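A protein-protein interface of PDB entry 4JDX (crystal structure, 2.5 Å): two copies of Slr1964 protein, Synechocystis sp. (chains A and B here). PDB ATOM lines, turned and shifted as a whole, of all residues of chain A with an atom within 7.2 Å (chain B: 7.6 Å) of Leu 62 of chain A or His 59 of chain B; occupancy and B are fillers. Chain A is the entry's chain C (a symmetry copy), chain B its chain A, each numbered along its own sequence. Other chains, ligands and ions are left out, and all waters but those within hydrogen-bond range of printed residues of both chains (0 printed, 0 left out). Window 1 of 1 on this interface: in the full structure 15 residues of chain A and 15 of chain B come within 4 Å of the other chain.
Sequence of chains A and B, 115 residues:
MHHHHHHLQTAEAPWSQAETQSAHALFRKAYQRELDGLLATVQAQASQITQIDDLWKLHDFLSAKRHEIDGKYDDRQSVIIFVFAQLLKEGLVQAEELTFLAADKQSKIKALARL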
ATOM      1  N   LEU A  38       8.395  11.072  -4.291  1.00  0.00           N
ATOM      2  CA  LEU A  38       8.316   9.618  -4.223  1.00  0.00           C
ATOM      3  C   LEU A  38       6.894   9.196  -3.870  1.00  0.00           C
ATOM      4  O   LEU A  38       6.332   8.284  -4.474  1.00  0.00           O
ATOM      5  CB  LEU A  38       9.287   9.091  -3.168  1.00  0.00           C
ATOM      6  CG  LEU A  38       9.314   7.575  -2.959  1.00  0.00           C
ATOM      7  CD1 LEU A  38       9.858   6.873  -4.197  1.00  0.00           C
ATOM      8  CD2 LEU A  38      10.128   7.226  -1.719  1.00  0.00           C
ATOM      9  N   VAL A  42       4.112   7.064  -6.182  1.00  0.00           N
ATOM     10  CA  VAL A  42       3.606   5.775  -5.727  1.00  0.00           C
ATOM     11  C   VAL A  42       2.081   5.767  -5.690  1.00  0.00           C
ATOM     12  O   VAL A  42       1.446   4.827  -6.166  1.00  0.00           O
ATOM     13  CB  VAL A  42       4.145   5.417  -4.326  1.00  0.00           C
ATOM     14  CG1 VAL A  42       3.429   4.186  -3.770  1.00  0.00           C
ATOM     15  CG2 VAL A  42       5.654   5.195  -4.381  1.00  0.00           C
ATOM     16  N   GLN A  45       0.930   5.737  -9.372  1.00  0.00           N
ATOM     17  CA  GLN A  45       1.141   4.427  -9.981  1.00  0.00           C
ATOM     18  C   GLN A  45       0.136   3.415  -9.452  1.00  0.00           C
ATOM     19  O   GLN A  45      -0.404   2.607 -10.207  1.00  0.00           O
ATOM     20  CB  GLN A  45       2.551   3.913  -9.683  1.00  0.00           C
ATOM     21  CG  GLN A  45       3.606   4.308 -10.693  1.00  0.00           C
ATOM     22  CD  GLN A  45       4.861   3.466 -10.569  1.00  0.00           C
ATOM     23  OE1 GLN A  45       4.791   2.243 -10.456  1.00  0.00           O
ATOM     24  NE2 GLN A  45       6.017   4.115 -10.580  1.00  0.00           N
ATOM     25  N   TRP A  56       4.057  -5.009 -10.256  1.00  0.00           N
ATOM     26  CA  TRP A  56       5.437  -5.461 -10.134  1.00  0.00           C
ATOM     27  C   TRP A  56       6.400  -4.329 -10.468  1.00  0.00           C
ATOM     28  O   TRP A  56       7.475  -4.231  -9.883  1.00  0.00           O
ATOM     29  CB  TRP A  56       5.689  -6.670 -11.037  1.00  0.00           C
ATOM     30  CG  TRP A  56       4.778  -7.829 -10.745  1.00  0.00           C
ATOM     31  CD1 TRP A  56       4.165  -8.638 -11.657  1.00  0.00           C
ATOM     32  CD2 TRP A  56       4.366  -8.300  -9.454  1.00  0.00           C
ATOM     33  NE1 TRP A  56       3.405  -9.584 -11.018  1.00  0.00           N
ATOM     34  CE2 TRP A  56       3.510  -9.399  -9.665  1.00  0.00           C
ATOM     35  CE3 TRP A  56       4.639  -7.903  -8.142  1.00  0.00           C
ATOM     36  CZ2 TRP A  56       2.927 -10.103  -8.617  1.00  0.00           C
ATOM     37  CZ3 TRP A  56       4.057  -8.606  -7.102  1.00  0.00           C
ATOM     38  CH2 TRP A  56       3.212  -9.692  -7.346  1.00  0.00           C
ATOM     39  N   LYS A  57       6.008  -3.477 -11.410  1.00  0.00           N
ATOM     40  CA  LYS A  57       6.793  -2.298 -11.752  1.00  0.00           C
ATOM     41  C   LYS A  57       6.895  -1.370 -10.552  1.00  0.00           C
ATOM     42  O   LYS A  57       7.976  -0.880 -10.221  1.00  0.00           O
ATOM     43  CB  LYS A  57       6.144  -1.544 -12.909  1.00  0.00           C
ATOM     44  CG  LYS A  57       6.267  -2.226 -14.255  1.00  0.00           C
ATOM     45  CD  LYS A  57       5.630  -1.378 -15.336  1.00  0.00           C
ATOM     46  CE  LYS A  57       5.626  -2.083 -16.676  1.00  0.00           C
ATOM     47  NZ  LYS A  57       5.008  -1.227 -17.724  1.00  0.00           N
ATOM     48  N   LEU A  58       5.756  -1.129  -9.910  1.00  0.00           N
ATOM     49  CA  LEU A  58       5.701  -0.275  -8.731  1.00  0.00           C
ATOM     50  C   LEU A  58       6.644  -0.801  -7.660  1.00  0.00           C
ATOM     51  O   LEU A  58       7.357  -0.038  -7.007  1.00  0.00           O
ATOM     52  CB  LEU A  58       4.276  -0.224  -8.179  1.00  0.00           C
ATOM     53  CG  LEU A  58       4.107   0.526  -6.856  1.00  0.00           C
ATOM     54  CD1 LEU A  58       4.652   1.951  -6.968  1.00  0.00           C
ATOM     55  CD2 LEU A  58       2.645   0.522  -6.426  1.00  0.00           C
ATOM     56  N   HIS A  59       6.641  -2.117  -7.492  1.00  0.00           N
ATOM     57  CA  HIS A  59       7.462  -2.773  -6.485  1.00  0.00           C
ATOM     58  C   HIS A  59       8.949  -2.591  -6.783  1.00  0.00           C
ATOM     59  O   HIS A  59       9.741  -2.299  -5.886  1.00  0.00           O
ATOM     60  CB  HIS A  59       7.116  -4.260  -6.433  1.00  0.00           C
ATOM     61  CG  HIS A  59       7.969  -5.049  -5.492  1.00  0.00           C
ATOM     62  ND1 HIS A  59       8.874  -5.995  -5.927  1.00  0.00           N
ATOM     63  CD2 HIS A  59       8.060  -5.039  -4.141  1.00  0.00           C
ATOM     64  CE1 HIS A  59       9.481  -6.534  -4.887  1.00  0.00           C
ATOM     65  NE2 HIS A  59       9.006  -5.970  -3.789  1.00  0.00           N
ATOM     66  N   ASP A  60       9.318  -2.765  -8.047  1.00  0.00           N
ATOM     67  CA  ASP A  60      10.701  -2.612  -8.474  1.00  0.00           C
ATOM     68  C   ASP A  60      11.142  -1.163  -8.305  1.00  0.00           C
ATOM     69  O   ASP A  60      12.280  -0.882  -7.925  1.00  0.00           O
ATOM     70  CB  ASP A  60      10.849  -3.031  -9.938  1.00  0.00           C
ATOM     71  CG  ASP A  60      10.604  -4.511 -10.150  1.00  0.00           C
ATOM     72  OD1 ASP A  60      10.688  -5.279  -9.169  1.00  0.00           O
ATOM     73  OD2 ASP A  60      10.338  -4.907 -11.303  1.00  0.00           O
ATOM     74  N   PHE A  61      10.223  -0.249  -8.595  1.00  0.00           N
ATOM     75  CA  PHE A  61      10.480   1.178  -8.468  1.00  0.00           C
ATOM     76  C   PHE A  61      10.783   1.541  -7.016  1.00  0.00           C
ATOM     77  O   PHE A  61      11.771   2.219  -6.731  1.00  0.00           O
ATOM     78  CB  PHE A  61       9.274   1.974  -8.975  1.00  0.00           C
ATOM     79  CG  PHE A  61       9.337   3.441  -8.656  1.00  0.00           C
ATOM     80  CD1 PHE A  61      10.060   4.309  -9.452  1.00  0.00           C
ATOM     81  CD2 PHE A  61       8.668   3.951  -7.557  1.00  0.00           C
ATOM     82  CE1 PHE A  61      10.117   5.656  -9.157  1.00  0.00           C
ATOM     83  CE2 PHE A  61       8.723   5.297  -7.259  1.00  0.00           C
ATOM     84  CZ  PHE A  61       9.447   6.149  -8.060  1.00  0.00           C
ATOM     85  N   LEU A  62       9.924   1.086  -6.108  1.00  0.00           N
ATOM     86  CA  LEU A  62      10.130   1.279  -4.677  1.00  0.00           C
ATOM     87  C   LEU A  62      11.450   0.670  -4.221  1.00  0.00           C
ATOM     88  O   LEU A  62      12.203   1.286  -3.466  1.00  0.00           O
ATOM     89  CB  LEU A  62       8.987   0.646  -3.884  1.00  0.00           C
ATOM     90  CG  LEU A  62       7.769   1.531  -3.620  1.00  0.00           C
ATOM     91  CD1 LEU A  62       6.587   0.692  -3.148  1.00  0.00           C
ATOM     92  CD2 LEU A  62       8.118   2.609  -2.600  1.00  0.00           C
ATOM     93  N   SER A  63      11.721  -0.548  -4.678  1.00  0.00           N
ATOM     94  CA  SER A  63      12.951  -1.243  -4.324  1.00  0.00           C
ATOM     95  C   SER A  63      14.158  -0.385  -4.682  1.00  0.00           C
ATOM     96  O   SER A  63      15.060  -0.183  -3.866  1.00  0.00           O
ATOM     97  CB  SER A  63      13.054  -2.577  -5.069  1.00  0.00           C
ATOM     98  OG  SER A  63      12.079  -3.518  -4.638  1.00  0.00           O
ATOM     99  N   ALA A  64      14.157   0.118  -5.913  1.00  0.00           N
ATOM    100  CA  ALA A  64      15.279   0.872  -6.455  1.00  0.00           C
ATOM    101  C   ALA A  64      15.483   2.184  -5.709  1.00  0.00           C
ATOM    102  O   ALA A  64      16.596   2.503  -5.288  1.00  0.00           O
ATOM    103  CB  ALA A  64      15.059   1.143  -7.943  1.00  0.00           C
ATOM    104  N   LYS A  65      14.403   2.941  -5.545  1.00  0.00           N
ATOM    105  CA  LYS A  65      14.474   4.258  -4.926  1.00  0.00           C
ATOM    106  C   LYS A  65      14.841   4.187  -3.451  1.00  0.00           C
ATOM    107  O   LYS A  65      15.595   5.022  -2.955  1.00  0.00           O
ATOM    108  CB  LYS A  65      13.146   4.999  -5.092  1.00  0.00           C
ATOM    109  CG  LYS A  65      13.020   5.722  -6.418  1.00  0.00           C
ATOM    110  CD  LYS A  65      14.021   6.860  -6.503  1.00  0.00           C
ATOM    111  CE  LYS A  65      13.940   7.593  -7.826  1.00  0.00           C
ATOM    112  NZ  LYS A  65      14.965   8.671  -7.913  1.00  0.00           N
ATOM    113  N   ARG A  66      14.311   3.193  -2.750  1.00  0.00           N
ATOM    114  CA  ARG A  66      14.593   3.056  -1.330  1.00  0.00           C
ATOM    115  C   ARG A  66      16.081   2.795  -1.116  1.00  0.00           C
ATOM    116  O   ARG A  66      16.676   3.291  -0.161  1.00  0.00           O
ATOM    117  CB  ARG A  66      13.764   1.933  -0.715  1.00  0.00           C
ATOM    118  CG  ARG A  66      13.907   1.849   0.790  1.00  0.00           C
ATOM    119  CD  ARG A  66      12.893   0.908   1.405  1.00  0.00           C
ATOM    120  NE  ARG A  66      13.027   0.847   2.859  1.00  0.00           N
ATOM    121  CZ  ARG A  66      12.095   0.374   3.681  1.00  0.00           C
ATOM    122  NH1 ARG A  66      10.945  -0.075   3.203  1.00  0.00           N
ATOM    123  NH2 ARG A  66      12.314   0.359   4.988  1.00  0.00           N
ATOM    124  N   HIS A  67      16.674   2.013  -2.012  1.00  0.00           N
ATOM    125  CA  HIS A  67      18.108   1.760  -1.973  1.00  0.00           C
ATOM    126  C   HIS A  67      18.873   3.043  -2.268  1.00  0.00           C
ATOM    127  O   HIS A  67      19.694   3.492  -1.469  1.00  0.00           O
ATOM    128  CB  HIS A  67      18.492   0.694  -2.999  1.00  0.00           C
ATOM    129  CG  HIS A  67      18.194  -0.706  -2.559  1.00  0.00           C
ATOM    130  ND1 HIS A  67      17.322  -1.529  -3.237  1.00  0.00           N
ATOM    131  CD2 HIS A  67      18.658  -1.428  -1.512  1.00  0.00           C
ATOM    132  CE1 HIS A  67      17.260  -2.699  -2.627  1.00  0.00           C
ATOM    133  NE2 HIS A  67      18.060  -2.664  -1.577  1.00  0.00           N
ATOM    134  N   GLU A  68      18.593   3.621  -3.430  1.00  0.00           N
ATOM    135  CA  GLU A  68      19.219   4.862  -3.856  1.00  0.00           C
ATOM    136  C   GLU A  68      19.238   5.874  -2.718  1.00  0.00           C
ATOM    137  O   GLU A  68      20.262   6.501  -2.444  1.00  0.00           O
ATOM    138  CB  GLU A  68      18.450   5.445  -5.043  1.00  0.00           C
ATOM    139  CG  GLU A  68      18.934   6.812  -5.491  1.00  0.00           C
ATOM    140  CD  GLU A  68      17.997   7.459  -6.490  1.00  0.00           C
ATOM    141  OE1 GLU A  68      17.216   6.728  -7.135  1.00  0.00           O
ATOM    142  OE2 GLU A  68      18.035   8.699  -6.628  1.00  0.00           O
ATOM    143  N   VAL B  42      -3.181  -3.489  -1.698  1.00  0.00           N
ATOM    144  CA  VAL B  42      -2.133  -2.551  -2.078  1.00  0.00           C
ATOM    145  C   VAL B  42      -2.739  -1.224  -2.511  1.00  0.00           C
ATOM    146  O   VAL B  42      -2.346  -0.158  -2.034  1.00  0.00           O
ATOM    147  CB  VAL B  42      -1.292  -3.112  -3.243  1.00  0.00           C
ATOM    148  CG1 VAL B  42      -0.390  -2.029  -3.849  1.00  0.00           C
ATOM    149  CG2 VAL B  42      -0.477  -4.309  -2.775  1.00  0.00           C
ATOM    150  N   GLN B  45      -4.213   0.510   0.847  1.00  0.00           N
ATOM    151  CA  GLN B  45      -3.331   1.047   1.876  1.00  0.00           C
ATOM    152  C   GLN B  45      -2.338   2.050   1.290  1.00  0.00           C
ATOM    153  O   GLN B  45      -1.550   2.654   2.017  1.00  0.00           O
ATOM    154  CB  GLN B  45      -2.598  -0.079   2.615  1.00  0.00           C
ATOM    155  CG  GLN B  45      -1.657  -0.896   1.755  1.00  0.00           C
ATOM    156  CD  GLN B  45      -0.886  -1.934   2.553  1.00  0.00           C
ATOM    157  OE1 GLN B  45      -1.071  -3.137   2.369  1.00  0.00           O
ATOM    158  NE2 GLN B  45      -0.011  -1.472   3.440  1.00  0.00           N
ATOM    159  N   ILE B  49      -2.257   6.305   2.685  1.00  0.00           N
ATOM    160  CA  ILE B  49      -0.950   6.784   3.106  1.00  0.00           C
ATOM    161  C   ILE B  49      -0.998   8.250   3.502  1.00  0.00           C
ATOM    162  O   ILE B  49      -1.556   9.085   2.791  1.00  0.00           O
ATOM    163  CB  ILE B  49       0.100   6.615   2.001  1.00  0.00           C
ATOM    164  CG1 ILE B  49       0.365   5.129   1.754  1.00  0.00           C
ATOM    165  CG2 ILE B  49       1.388   7.337   2.383  1.00  0.00           C
ATOM    166  CD1 ILE B  49       1.473   4.858   0.755  1.00  0.00           C
ATOM    167  N   ASP B  53       6.365   6.433   6.523  1.00  0.00           N
ATOM    168  CA  ASP B  53       6.614   5.083   6.997  1.00  0.00           C
ATOM    169  C   ASP B  53       5.494   4.158   6.535  1.00  0.00           C
ATOM    170  O   ASP B  53       5.697   2.957   6.389  1.00  0.00           O
ATOM    171  CB  ASP B  53       6.757   5.062   8.519  1.00  0.00           C
ATOM    172  CG  ASP B  53       7.928   5.896   9.002  1.00  0.00           C
ATOM    173  OD1 ASP B  53       9.062   5.374   9.018  1.00  0.00           O
ATOM    174  OD2 ASP B  53       7.715   7.073   9.359  1.00  0.00           O
ATOM    175  N   ASP B  54       4.318   4.730   6.288  1.00  0.00           N
ATOM    176  CA  ASP B  54       3.209   3.987   5.699  1.00  0.00           C
ATOM    177  C   ASP B  54       3.633   3.431   4.349  1.00  0.00           C
ATOM    178  O   ASP B  54       3.231   2.334   3.959  1.00  0.00           O
ATOM    179  CB  ASP B  54       1.996   4.898   5.499  1.00  0.00           C
ATOM    180  CG  ASP B  54       1.356   5.320   6.802  1.00  0.00           C
ATOM    181  OD1 ASP B  54       1.484   4.579   7.797  1.00  0.00           O
ATOM    182  OD2 ASP B  54       0.719   6.394   6.826  1.00  0.00           O
ATOM    183  N   LEU B  55       4.447   4.206   3.641  1.00  0.00           N
ATOM    184  CA  LEU B  55       4.916   3.834   2.314  1.00  0.00           C
ATOM    185  C   LEU B  55       5.985   2.748   2.396  1.00  0.00           C
ATOM    186  O   LEU B  55       6.115   1.925   1.490  1.00  0.00           O
ATOM    187  CB  LEU B  55       5.453   5.073   1.591  1.00  0.00           C
ATOM    188  CG  LEU B  55       5.933   4.925   0.147  1.00  0.00           C
ATOM    189  CD1 LEU B  55       5.713   6.231  -0.606  1.00  0.00           C
ATOM    190  CD2 LEU B  55       7.403   4.522   0.112  1.00  0.00           C
ATOM    191  N   TRP B  56       6.743   2.741   3.488  1.00  0.00           N
ATOM    192  CA  TRP B  56       7.769   1.724   3.697  1.00  0.00           C
ATOM    193  C   TRP B  56       7.147   0.428   4.211  1.00  0.00           C
ATOM    194  O   TRP B  56       7.622  -0.664   3.899  1.00  0.00           O
ATOM    195  CB  TRP B  56       8.838   2.224   4.673  1.00  0.00           C
ATOM    196  CG  TRP B  56       9.556   3.469   4.211  1.00  0.00           C
ATOM    197  CD1 TRP B  56       9.769   4.609   4.931  1.00  0.00           C
ATOM    198  CD2 TRP B  56      10.148   3.695   2.925  1.00  0.00           C
ATOM    199  NE1 TRP B  56      10.459   5.526   4.177  1.00  0.00           N
ATOM    200  CE2 TRP B  56      10.702   4.990   2.941  1.00  0.00           C
ATOM    201  CE3 TRP B  56      10.263   2.928   1.762  1.00  0.00           C
ATOM    202  CZ2 TRP B  56      11.361   5.535   1.841  1.00  0.00           C
ATOM    203  CZ3 TRP B  56      10.918   3.471   0.673  1.00  0.00           C
ATOM    204  CH2 TRP B  56      11.457   4.761   0.721  1.00  0.00           C
ATOM    205  N   LYS B  57       6.085   0.555   4.998  1.00  0.00           N
ATOM    206  CA  LYS B  57       5.346  -0.608   5.475  1.00  0.00           C
ATOM    207  C   LYS B  57       4.724  -1.332   4.291  1.00  0.00           C
ATOM    208  O   LYS B  57       4.744  -2.560   4.217  1.00  0.00           O
ATOM    209  CB  LYS B  57       4.249  -0.185   6.449  1.00  0.00           C
ATOM    210  CG  LYS B  57       4.761   0.294   7.790  1.00  0.00           C
ATOM    211  CD  LYS B  57       3.617   0.554   8.751  1.00  0.00           C
ATOM    212  CE  LYS B  57       4.100   1.223  10.025  1.00  0.00           C
ATOM    213  NZ  LYS B  57       4.402   2.662   9.803  1.00  0.00           N
ATOM    214  N   LEU B  58       4.172  -0.554   3.366  1.00  0.00           N
ATOM    215  CA  LEU B  58       3.577  -1.097   2.153  1.00  0.00           C
ATOM    216  C   LEU B  58       4.641  -1.809   1.337  1.00  0.00           C
ATOM    217  O   LEU B  58       4.420  -2.898   0.809  1.00  0.00           O
ATOM    218  CB  LEU B  58       2.960   0.025   1.321  1.00  0.00           C
ATOM    219  CG  LEU B  58       2.537  -0.355  -0.100  1.00  0.00           C
ATOM    220  CD1 LEU B  58       1.422  -1.400  -0.078  1.00  0.00           C
ATOM    221  CD2 LEU B  58       2.121   0.890  -0.875  1.00  0.00           C
ATOM    222  N   HIS B  59       5.803  -1.178   1.234  1.00  0.00           N
ATOM    223  CA  HIS B  59       6.922  -1.754   0.509  1.00  0.00           C
ATOM    224  C   HIS B  59       7.317  -3.104   1.096  1.00  0.00           C
ATOM    225  O   HIS B  59       7.532  -4.072   0.365  1.00  0.00           O
ATOM    226  CB  HIS B  59       8.117  -0.810   0.554  1.00  0.00           C
ATOM    227  CG  HIS B  59       9.357  -1.388  -0.052  1.00  0.00           C
ATOM    228  ND1 HIS B  59       9.487  -1.605  -1.404  1.00  0.00           N
ATOM    229  CD2 HIS B  59      10.511  -1.809   0.515  1.00  0.00           C
ATOM    230  CE1 HIS B  59      10.678  -2.126  -1.649  1.00  0.00           C
ATOM    231  NE2 HIS B  59      11.318  -2.260  -0.504  1.00  0.00           N
ATOM    232  N   ASP B  60       7.412  -3.162   2.421  1.00  0.00           N
ATOM    233  CA  ASP B  60       7.779  -4.393   3.110  1.00  0.00           C
ATOM    234  C   ASP B  60       6.743  -5.472   2.830  1.00  0.00           C
ATOM    235  O   ASP B  60       7.080  -6.637   2.613  1.00  0.00           O
ATOM    236  CB  ASP B  60       7.877  -4.152   4.618  1.00  0.00           C
ATOM    237  CG  ASP B  60       8.997  -3.198   4.988  1.00  0.00           C
ATOM    238  OD1 ASP B  60       9.940  -3.038   4.184  1.00  0.00           O
ATOM    239  OD2 ASP B  60       8.934  -2.614   6.090  1.00  0.00           O
ATOM    240  N   PHE B  61       5.477  -5.069   2.838  1.00  0.00           N
ATOM    241  CA  PHE B  61       4.365  -5.974   2.576  1.00  0.00           C
ATOM    242  C   PHE B  61       4.472  -6.605   1.187  1.00  0.00           C
ATOM    243  O   PHE B  61       4.354  -7.821   1.044  1.00  0.00           O
ATOM    244  CB  PHE B  61       3.038  -5.224   2.721  1.00  0.00           C
ATOM    245  CG  PHE B  61       1.836  -6.019   2.290  1.00  0.00           C
ATOM    246  CD1 PHE B  61       1.271  -6.960   3.128  1.00  0.00           C
ATOM    247  CD2 PHE B  61       1.266  -5.815   1.046  1.00  0.00           C
ATOM    248  CE1 PHE B  61       0.167  -7.689   2.731  1.00  0.00           C
ATOM    249  CE2 PHE B  61       0.162  -6.540   0.647  1.00  0.00           C
ATOM    250  CZ  PHE B  61      -0.388  -7.477   1.490  1.00  0.00           C
ATOM    251  N   LEU B  62       4.697  -5.778   0.169  1.00  0.00           N
ATOM    252  CA  LEU B  62       4.844  -6.264  -1.204  1.00  0.00           C
ATOM    253  C   LEU B  62       6.036  -7.200  -1.352  1.00  0.00           C
ATOM    254  O   LEU B  62       5.936  -8.249  -1.988  1.00  0.00           O
ATOM    255  CB  LEU B  62       5.008  -5.094  -2.175  1.00  0.00           C
ATOM    256  CG  LEU B  62       3.724  -4.435  -2.674  1.00  0.00           C
ATOM    257  CD1 LEU B  62       4.043  -3.098  -3.329  1.00  0.00           C
ATOM    258  CD2 LEU B  62       2.995  -5.359  -3.644  1.00  0.00           C
ATOM    259  N   SER B  63       7.168  -6.806  -0.778  1.00  0.00           N
ATOM    260  CA  SER B  63       8.377  -7.616  -0.844  1.00  0.00           C
ATOM    261  C   SER B  63       8.088  -9.013  -0.321  1.00  0.00           C
ATOM    262  O   SER B  63       8.508 -10.011  -0.909  1.00  0.00           O
ATOM    263  CB  SER B  63       9.498  -6.988  -0.013  1.00  0.00           C
ATOM    264  OG  SER B  63      10.066  -5.844  -0.643  1.00  0.00           O
ATOM    265  N   ALA B  64       7.356  -9.071   0.784  1.00  0.00           N
ATOM    266  CA  ALA B  64       7.092 -10.323   1.479  1.00  0.00           C
ATOM    267  C   ALA B  64       6.047 -11.143   0.736  1.00  0.00           C
ATOM    268  O   ALA B  64       6.245 -12.331   0.478  1.00  0.00           O
ATOM    269  CB  ALA B  64       6.629 -10.044   2.904  1.00  0.00           C
ATOM    270  N   LYS B  65       4.935 -10.502   0.391  1.00  0.00           N
ATOM    271  CA  LYS B  65       3.831 -11.191  -0.264  1.00  0.00           C
ATOM    272  C   LYS B  65       4.268 -11.710  -1.627  1.00  0.00           C
ATOM    273  O   LYS B  65       3.769 -12.729  -2.100  1.00  0.00           O
ATOM    274  CB  LYS B  65       2.625 -10.263  -0.419  1.00  0.00           C
ATOM    275  CG  LYS B  65       1.284 -10.964  -0.248  1.00  0.00           C
ATOM    276  CD  LYS B  65       1.071 -11.412   1.192  1.00  0.00           C
ATOM    277  CE  LYS B  65      -0.338 -11.942   1.420  1.00  0.00           C
ATOM    278  NZ  LYS B  65      -0.653 -13.110   0.551  1.00  0.00           N
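The backbone carbonyl oxygen (O) of Trp 56 of chain B lies close to the guanidinium group (NH1) of Arg 66 of chain A (3.4 Å).
The side-chain carboxylate (OD1) of Asp 60 of chain B is in salt-bridge range of the guanidinium group (NH1) of Arg 66 of chain A, 3.3 Å away.
The side-chain hydroxyl (OG) of Ser 63 of chain B lies within hydrogen-bond range of a ring nitrogen (NE2) of His 59 of chain A (3.3 Å).
The backbone carbonyl oxygen of His 59 of chain B sits at hydrogen-bond distance from the side-chain hydroxyl of Ser 63 of chain B (3.3 Å).
O of His 59 of chain A sits at hydrogen-bond distance from OG of Ser 63 of chain A (2.9 Å).
The backbone carbonyl oxygen (O) of Ser 63 of chain A sits at hydrogen-bond distance from a ring nitrogen (ND1) of His 67 of chain A (2.7 Å).
Among the printed residues, pairs that only touch across the chains: Arg 66 of chain A with His 59 of chain B, Leu 62 of chain A with His 59 of chain B, Leu 62 of chain A with Leu 55 of chain B, Ser 63 of chain A with His 59 of chain B, His 59 of chain A with Leu 62 of chain B, Leu 38 of chain A with Trp 56 of chain B and Val 42 of chain A with Leu 55 of chain B.
Leu 62 of chain A touches just these residues of chain B: Leu 55 and His 59.
Printed residues of chain A within 4 Å of Leu 55 of chain B: Val 42 (3.9 Å) and Leu 62 (3.4 Å).
Of chain A, only Leu 62, Ser 63 and Arg 66 come within 4 Å of His 59 of chain B.
Of the printed residues of chain A, Leu 62 of chain B touches His 59 (3.6 Å).
The nearest residue of chain A that does not touch His 59 of chain B is His 59 of chain A (4.3 Å).
Printed residues of chain B that touch a printed residue of chain A: Leu 55, Trp 56, His 59, Asp 60, Leu 62 and Ser 63.
Hydrophobic or aromatic side chains of chain B within 4 Å of the printed part of chain A: Leu 55, Trp 56, His 59 and Leu 62.
Printed residues of chain A that touch a printed residue of chain B: Leu 38, Val 42, His 59, Leu 62, Ser 63 and Arg 66.
Hydrophobic or aromatic side chains of chain A within 4 Å of the printed part of chain B: Leu 38, Val 42, His 59 and Leu 62.
Among the printed residues, Asp or Glu carboxylates within 4 Å of a Lys or Arg side-chain nitrogen of the other chain: Arg 66 of chain A with Asp 60 of chain B.
His 59 of chain A touches Leu 62 of chain B, and with the chains exchanged Leu 62 of chain A touches His 59 of chain B.
His 59 of chain A touches Ser 63 of chain B, and with the chains exchanged Ser 63 of chain A touches His 59 of chain B.
12 positions are printed for both chains.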
